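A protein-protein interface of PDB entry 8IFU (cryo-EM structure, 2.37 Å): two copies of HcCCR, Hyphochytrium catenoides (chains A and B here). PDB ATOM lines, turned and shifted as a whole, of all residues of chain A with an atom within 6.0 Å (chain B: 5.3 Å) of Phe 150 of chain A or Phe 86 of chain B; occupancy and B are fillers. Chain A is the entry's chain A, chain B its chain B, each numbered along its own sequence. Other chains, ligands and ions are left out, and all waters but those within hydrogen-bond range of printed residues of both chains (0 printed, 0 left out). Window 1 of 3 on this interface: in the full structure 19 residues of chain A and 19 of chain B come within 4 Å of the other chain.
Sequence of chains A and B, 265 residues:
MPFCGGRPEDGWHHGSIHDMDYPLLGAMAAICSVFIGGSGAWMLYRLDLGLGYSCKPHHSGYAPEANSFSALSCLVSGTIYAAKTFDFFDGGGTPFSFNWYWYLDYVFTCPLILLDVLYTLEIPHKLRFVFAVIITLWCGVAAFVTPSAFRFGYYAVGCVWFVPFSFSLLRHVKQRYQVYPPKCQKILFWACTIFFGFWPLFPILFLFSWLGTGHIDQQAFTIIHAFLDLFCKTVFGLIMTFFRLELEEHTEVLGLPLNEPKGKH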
ATOM      1  N   ALA A 143      -7.671 -20.153  27.601  1.00  0.00           N
ATOM      2  CA  ALA A 143      -7.505 -21.512  27.134  1.00  0.00           C
ATOM      3  C   ALA A 143      -8.117 -21.771  25.783  1.00  0.00           C
ATOM      4  O   ALA A 143      -7.618 -22.585  25.022  1.00  0.00           O
ATOM      5  CB  ALA A 143      -8.102 -22.452  28.136  1.00  0.00           C
ATOM      6  N   THR A 146      -5.619 -19.802  23.181  1.00  0.00           N
ATOM      7  CA  THR A 146      -4.273 -20.325  22.959  1.00  0.00           C
ATOM      8  C   THR A 146      -4.242 -21.508  22.032  1.00  0.00           C
ATOM      9  O   THR A 146      -4.940 -22.488  22.247  1.00  0.00           O
ATOM     10  CB  THR A 146      -3.522 -20.713  24.252  1.00  0.00           C
ATOM     11  OG1 THR A 146      -4.408 -20.690  25.361  1.00  0.00           O
ATOM     12  CG2 THR A 146      -2.387 -19.773  24.513  1.00  0.00           C
ATOM     13  N   SER A 148      -1.751 -23.600  21.511  1.00  0.00           N
ATOM     14  CA  SER A 148      -0.721 -24.552  21.862  1.00  0.00           C
ATOM     15  C   SER A 148      -1.162 -25.380  23.032  1.00  0.00           C
ATOM     16  O   SER A 148      -2.287 -25.272  23.464  1.00  0.00           O
ATOM     17  CB  SER A 148       0.535 -23.798  22.246  1.00  0.00           C
ATOM     18  OG  SER A 148       0.217 -22.596  22.918  1.00  0.00           O
ATOM     19  N   ALA A 149      -0.261 -26.182  23.585  1.00  0.00           N
ATOM     20  CA  ALA A 149      -0.565 -26.976  24.763  1.00  0.00           C
ATOM     21  C   ALA A 149      -0.450 -26.161  26.022  1.00  0.00           C
ATOM     22  O   ALA A 149      -0.533 -26.700  27.104  1.00  0.00           O
ATOM     23  CB  ALA A 149       0.338 -28.170  24.820  1.00  0.00           C
ATOM     24  N   PHE A 150      -0.273 -24.856  25.894  1.00  0.00           N
ATOM     25  CA  PHE A 150      -0.236 -23.967  27.033  1.00  0.00           C
ATOM     26  C   PHE A 150      -1.651 -23.589  27.332  1.00  0.00           C
ATOM     27  O   PHE A 150      -1.890 -22.864  28.273  1.00  0.00           O
ATOM     28  CB  PHE A 150       0.620 -22.753  26.730  1.00  0.00           C
ATOM     29  CG  PHE A 150       2.079 -22.975  26.960  1.00  0.00           C
ATOM     30  CD1 PHE A 150       2.606 -22.910  28.233  1.00  0.00           C
ATOM     31  CD2 PHE A 150       2.923 -23.259  25.905  1.00  0.00           C
ATOM     32  CE1 PHE A 150       3.949 -23.118  28.451  1.00  0.00           C
ATOM     33  CE2 PHE A 150       4.266 -23.471  26.117  1.00  0.00           C
ATOM     34  CZ  PHE A 150       4.780 -23.400  27.391  1.00  0.00           C
ATOM     35  N   ARG A 151      -2.599 -24.096  26.558  1.00  0.00           N
ATOM     36  CA  ARG A 151      -4.008 -23.895  26.811  1.00  0.00           C
ATOM     37  C   ARG A 151      -4.379 -24.759  27.984  1.00  0.00           C
ATOM     38  O   ARG A 151      -5.309 -24.456  28.702  1.00  0.00           O
ATOM     39  CB  ARG A 151      -4.788 -24.308  25.564  1.00  0.00           C
ATOM     40  CG  ARG A 151      -5.292 -25.741  25.499  1.00  0.00           C
ATOM     41  CD  ARG A 151      -5.964 -26.058  24.179  1.00  0.00           C
ATOM     42  NE  ARG A 151      -4.981 -26.217  23.124  1.00  0.00           N
ATOM     43  CZ  ARG A 151      -4.786 -27.330  22.431  1.00  0.00           C
ATOM     44  NH1 ARG A 151      -3.853 -27.368  21.496  1.00  0.00           N
ATOM     45  NH2 ARG A 151      -5.516 -28.403  22.662  1.00  0.00           N
ATOM     46  N   PHE A 152      -3.607 -25.807  28.220  1.00  0.00           N
ATOM     47  CA  PHE A 152      -3.837 -26.699  29.315  1.00  0.00           C
ATOM     48  C   PHE A 152      -3.201 -26.150  30.546  1.00  0.00           C
ATOM     49  O   PHE A 152      -3.521 -26.589  31.631  1.00  0.00           O
ATOM     50  CB  PHE A 152      -3.287 -28.056  28.952  1.00  0.00           C
ATOM     51  CG  PHE A 152      -4.020 -28.712  27.825  1.00  0.00           C
ATOM     52  CD1 PHE A 152      -5.384 -28.923  27.903  1.00  0.00           C
ATOM     53  CD2 PHE A 152      -3.351 -29.104  26.685  1.00  0.00           C
ATOM     54  CE1 PHE A 152      -6.065 -29.521  26.867  1.00  0.00           C
ATOM     55  CE2 PHE A 152      -4.025 -29.703  25.646  1.00  0.00           C
ATOM     56  CZ  PHE A 152      -5.385 -29.915  25.738  1.00  0.00           C
ATOM     57  N   GLY A 153      -2.331 -25.168  30.401  1.00  0.00           N
ATOM     58  CA  GLY A 153      -1.764 -24.499  31.536  1.00  0.00           C
ATOM     59  C   GLY A 153      -2.729 -23.466  32.024  1.00  0.00           C
ATOM     60  O   GLY A 153      -2.891 -23.324  33.210  1.00  0.00           O
ATOM     61  N   TYR A 154      -3.388 -22.753  31.132  1.00  0.00           N
ATOM     62  CA  TYR A 154      -4.422 -21.804  31.541  1.00  0.00           C
ATOM     63  C   TYR A 154      -5.609 -22.538  32.112  1.00  0.00           C
ATOM     64  O   TYR A 154      -6.225 -22.083  33.056  1.00  0.00           O
ATOM     65  CB  TYR A 154      -4.885 -20.955  30.368  1.00  0.00           C
ATOM     66  CG  TYR A 154      -3.919 -19.937  29.876  1.00  0.00           C
ATOM     67  CD1 TYR A 154      -3.589 -18.838  30.646  1.00  0.00           C
ATOM     68  CD2 TYR A 154      -3.355 -20.054  28.625  1.00  0.00           C
ATOM     69  CE1 TYR A 154      -2.702 -17.891  30.185  1.00  0.00           C
ATOM     70  CE2 TYR A 154      -2.466 -19.120  28.159  1.00  0.00           C
ATOM     71  CZ  TYR A 154      -2.147 -18.038  28.940  1.00  0.00           C
ATOM     72  OH  TYR A 154      -1.263 -17.106  28.465  1.00  0.00           O
ATOM     73  N   TYR A 155      -5.923 -23.693  31.562  1.00  0.00           N
ATOM     74  CA  TYR A 155      -6.996 -24.498  32.078  1.00  0.00           C
ATOM     75  C   TYR A 155      -6.716 -24.953  33.475  1.00  0.00           C
ATOM     76  O   TYR A 155      -7.580 -24.867  34.330  1.00  0.00           O
ATOM     77  CB  TYR A 155      -7.207 -25.697  31.161  1.00  0.00           C
ATOM     78  CG  TYR A 155      -8.244 -26.679  31.620  1.00  0.00           C
ATOM     79  CD1 TYR A 155      -9.592 -26.363  31.581  1.00  0.00           C
ATOM     80  CD2 TYR A 155      -7.874 -27.927  32.085  1.00  0.00           C
ATOM     81  CE1 TYR A 155     -10.542 -27.268  32.000  1.00  0.00           C
ATOM     82  CE2 TYR A 155      -8.814 -28.831  32.512  1.00  0.00           C
ATOM     83  CZ  TYR A 155     -10.144 -28.498  32.461  1.00  0.00           C
ATOM     84  OH  TYR A 155     -11.066 -29.414  32.885  1.00  0.00           O
ATOM     85  N   VAL A 157      -4.696 -23.549  35.652  1.00  0.00           N
ATOM     86  CA  VAL A 157      -4.633 -22.433  36.574  1.00  0.00           C
ATOM     87  C   VAL A 157      -6.033 -22.062  37.035  1.00  0.00           C
ATOM     88  O   VAL A 157      -6.239 -21.724  38.186  1.00  0.00           O
ATOM     89  CB  VAL A 157      -3.796 -21.259  36.011  1.00  0.00           C
ATOM     90  CG1 VAL A 157      -4.015 -19.969  36.785  1.00  0.00           C
ATOM     91  CG2 VAL A 157      -2.323 -21.620  36.044  1.00  0.00           C
ATOM     92  N   ALA B  82       1.752 -16.269  36.016  1.00  0.00           N
ATOM     93  CA  ALA B  82       1.653 -17.616  35.462  1.00  0.00           C
ATOM     94  C   ALA B  82       1.290 -17.511  33.996  1.00  0.00           C
ATOM     95  O   ALA B  82       1.832 -18.221  33.188  1.00  0.00           O
ATOM     96  CB  ALA B  82       0.646 -18.438  36.231  1.00  0.00           C
ATOM     97  N   ALA B  83       0.415 -16.582  33.645  1.00  0.00           N
ATOM     98  CA  ALA B  83       0.075 -16.326  32.270  1.00  0.00           C
ATOM     99  C   ALA B  83       1.277 -15.808  31.535  1.00  0.00           C
ATOM    100  O   ALA B  83       1.473 -16.139  30.380  1.00  0.00           O
ATOM    101  CB  ALA B  83      -1.053 -15.332  32.205  1.00  0.00           C
ATOM    102  N   LYS B  84       2.085 -14.985  32.181  1.00  0.00           N
ATOM    103  CA  LYS B  84       3.307 -14.512  31.610  1.00  0.00           C
ATOM    104  C   LYS B  84       4.341 -15.599  31.369  1.00  0.00           C
ATOM    105  O   LYS B  84       5.002 -15.568  30.368  1.00  0.00           O
ATOM    106  CB  LYS B  84       3.880 -13.403  32.481  1.00  0.00           C
ATOM    107  CG  LYS B  84       3.113 -12.105  32.498  1.00  0.00           C
ATOM    108  CD  LYS B  84       3.659 -11.205  33.585  1.00  0.00           C
ATOM    109  CE  LYS B  84       3.110  -9.801  33.472  1.00  0.00           C
ATOM    110  NZ  LYS B  84       3.853  -8.830  34.315  1.00  0.00           N
ATOM    111  N   THR B  85       4.465 -16.581  32.255  1.00  0.00           N
ATOM    112  CA  THR B  85       5.373 -17.690  32.023  1.00  0.00           C
ATOM    113  C   THR B  85       4.931 -18.513  30.844  1.00  0.00           C
ATOM    114  O   THR B  85       5.757 -18.985  30.104  1.00  0.00           O
ATOM    115  CB  THR B  85       5.760 -18.567  33.288  1.00  0.00           C
ATOM    116  OG1 THR B  85       5.895 -19.940  32.915  1.00  0.00           O
ATOM    117  CG2 THR B  85       4.827 -18.513  34.365  1.00  0.00           C
ATOM    118  N   PHE B  86       3.628 -18.656  30.649  1.00  0.00           N
ATOM    119  CA  PHE B  86       3.102 -19.391  29.530  1.00  0.00           C
ATOM    120  C   PHE B  86       3.428 -18.695  28.233  1.00  0.00           C
ATOM    121  O   PHE B  86       3.813 -19.356  27.286  1.00  0.00           O
ATOM    122  CB  PHE B  86       1.601 -19.615  29.666  1.00  0.00           C
ATOM    123  CG  PHE B  86       1.189 -20.381  30.884  1.00  0.00           C
ATOM    124  CD1 PHE B  86       2.054 -21.264  31.512  1.00  0.00           C
ATOM    125  CD2 PHE B  86      -0.084 -20.222  31.396  1.00  0.00           C
ATOM    126  CE1 PHE B  86       1.660 -21.949  32.638  1.00  0.00           C
ATOM    127  CE2 PHE B  86      -0.478 -20.902  32.519  1.00  0.00           C
ATOM    128  CZ  PHE B  86       0.393 -21.770  33.140  1.00  0.00           C
ATOM    129  N   ASP B  87       3.285 -17.372  28.172  1.00  0.00           N
ATOM    130  CA  ASP B  87       3.684 -16.618  26.994  1.00  0.00           C
ATOM    131  C   ASP B  87       5.180 -16.655  26.722  1.00  0.00           C
ATOM    132  O   ASP B  87       5.588 -16.879  25.604  1.00  0.00           O
ATOM    133  CB  ASP B  87       3.163 -15.182  27.047  1.00  0.00           C
ATOM    134  CG  ASP B  87       3.801 -14.275  26.002  1.00  0.00           C
ATOM    135  OD1 ASP B  87       3.346 -14.272  24.855  1.00  0.00           O
ATOM    136  OD2 ASP B  87       4.760 -13.546  26.314  1.00  0.00           O
ATOM    137  N   PHE B  88       5.998 -16.448  27.728  1.00  0.00           N
ATOM    138  CA  PHE B  88       7.421 -16.491  27.550  1.00  0.00           C
ATOM    139  C   PHE B  88       7.922 -17.869  27.135  1.00  0.00           C
ATOM    140  O   PHE B  88       8.835 -17.978  26.356  1.00  0.00           O
ATOM    141  CB  PHE B  88       8.145 -16.057  28.821  1.00  0.00           C
ATOM    142  CG  PHE B  88       8.097 -14.598  29.128  1.00  0.00           C
ATOM    143  CD1 PHE B  88       8.270 -13.652  28.149  1.00  0.00           C
ATOM    144  CD2 PHE B  88       7.936 -14.178  30.434  1.00  0.00           C
ATOM    145  CE1 PHE B  88       8.263 -12.309  28.456  1.00  0.00           C
ATOM    146  CE2 PHE B  88       7.922 -12.843  30.753  1.00  0.00           C
ATOM    147  CZ  PHE B  88       8.099 -11.906  29.761  1.00  0.00           C
ATOM    148  N   PHE B  89       7.322 -18.929  27.643  1.00  0.00           N
ATOM    149  CA  PHE B  89       7.720 -20.286  27.284  1.00  0.00           C
ATOM    150  C   PHE B  89       7.175 -20.721  25.945  1.00  0.00           C
ATOM    151  O   PHE B  89       7.609 -21.723  25.414  1.00  0.00           O
ATOM    152  CB  PHE B  89       7.464 -21.275  28.415  1.00  0.00           C
ATOM    153  CG  PHE B  89       8.529 -21.294  29.458  1.00  0.00           C
ATOM    154  CD1 PHE B  89       9.858 -21.357  29.103  1.00  0.00           C
ATOM    155  CD2 PHE B  89       8.198 -21.263  30.795  1.00  0.00           C
ATOM    156  CE1 PHE B  89      10.840 -21.391  30.066  1.00  0.00           C
ATOM    157  CE2 PHE B  89       9.172 -21.298  31.762  1.00  0.00           C
ATOM    158  CZ  PHE B  89      10.497 -21.359  31.397  1.00  0.00           C
ATOM    159  N   ASP B  90       6.250 -19.964  25.377  1.00  0.00           N
ATOM    160  CA  ASP B  90       5.785 -20.212  24.037  1.00  0.00           C
ATOM    161  C   ASP B  90       6.536 -19.296  23.066  1.00  0.00           C
ATOM    162  O   ASP B  90       6.308 -19.368  21.873  1.00  0.00           O
ATOM    163  CB  ASP B  90       4.310 -19.967  23.974  1.00  0.00           C
ATOM    164  CG  ASP B  90       3.564 -21.042  23.253  1.00  0.00           C
ATOM    165  OD1 ASP B  90       4.201 -21.950  22.689  1.00  0.00           O
ATOM    166  OD2 ASP B  90       2.324 -20.974  23.252  1.00  0.00           O
ATOM    167  N   GLY B  91       7.414 -18.424  23.552  1.00  0.00           N
ATOM    168  CA  GLY B  91       8.242 -17.587  22.707  1.00  0.00           C
ATOM    169  C   GLY B  91       7.787 -16.194  22.466  1.00  0.00           C
ATOM    170  O   GLY B  91       8.314 -15.541  21.591  1.00  0.00           O
ATOM    171  N   THR B  94       1.669 -14.263  22.017  1.00  0.00           N
ATOM    172  CA  THR B  94       0.694 -15.303  21.934  1.00  0.00           C
ATOM    173  C   THR B  94      -0.596 -14.554  22.062  1.00  0.00           C
ATOM    174  O   THR B  94      -0.594 -13.444  22.536  1.00  0.00           O
ATOM    175  CB  THR B  94       0.939 -16.274  23.103  1.00  0.00           C
ATOM    176  OG1 THR B  94       1.156 -15.529  24.300  1.00  0.00           O
ATOM    177  CG2 THR B  94       2.135 -17.139  22.834  1.00  0.00           C
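The side-chain hydroxyl of Ser 148 of chain A sits at hydrogen-bond distance from the side-chain carboxylate of Asp 90 of chain B.
The side-chain hydroxyl (OH) of Tyr 154 of chain A is in hydrogen-bond range of the backbone carbonyl oxygen (O) of Ala 83 of chain B (3.5 Å).
Phe 150 of chain A touches just these residues of chain B: Phe 86 (3.7 Å), Phe 89 (3.6 Å) and Asp 90 (3.5 Å).
Of the printed residues of chain B, Gly 153 of chain A touches Phe 86.
Of the printed residues of chain A, Ala 83 of chain B touches Tyr 154.
Of chain A, only Phe 150 (3.7 Å), Gly 153 (3.4 Å), Tyr 154 (3.7 Å) and Val 157 (3.98 Å) come within 4 Å of Phe 86 of chain B.
Thr 94 of chain B touches none of the printed residues of chain A.
The nearest residue of chain B that does not touch Phe 150 of chain A is Thr 85 of chain B (4.8 Å).
Phe 86 of chain B touches Phe 150 of chain A (CD1 to CD1, 3.7 Å).
Phe 150 of chain A touches Phe 89 of chain B.
Phe 150 of chain A touches Asp 90 of chain B (CD2 to CG, 3.5 Å).
C of Gly 153 of chain A touches CE2 of Phe 86 of chain B, at 3.4 Å.
Phe 86 of chain B touches Tyr 154 of chain A.
Val 157 of chain A touches Phe 86 of chain B (CG2 to CZ, 3.98 Å).
No position is printed for both chains.
Of the 11 printed residues of chain B, 4 touch a printed residue of chain A.
Hydrophobic or aromatic side chains of chain B within 4 Å of the printed part of chain A: Ala 83, Phe 86 and Phe 89.
Along chain B the printed residues that touch a printed residue of chain A span positions 83 to 90.
Of the 11 printed residues of chain A, 5 touch a printed residue of chain B.
Hydrophobic or aromatic side chains of chain A within 4 Å of the printed part of chain B: Phe 150, Tyr 154 and Val 157.
Along chain A the printed residues that touch a printed residue of chain B span positions 148 to 157.
Among the printed residues, no Asp or Glu carboxylate lies within 4 Å of a Lys or Arg side-chain nitrogen of the other chain.
The backbone carbonyl oxygen of Ser 148 of chain A is in hydrogen-bond range of the guanidinium group of Arg 151 of chain A, 2.9 Å away.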
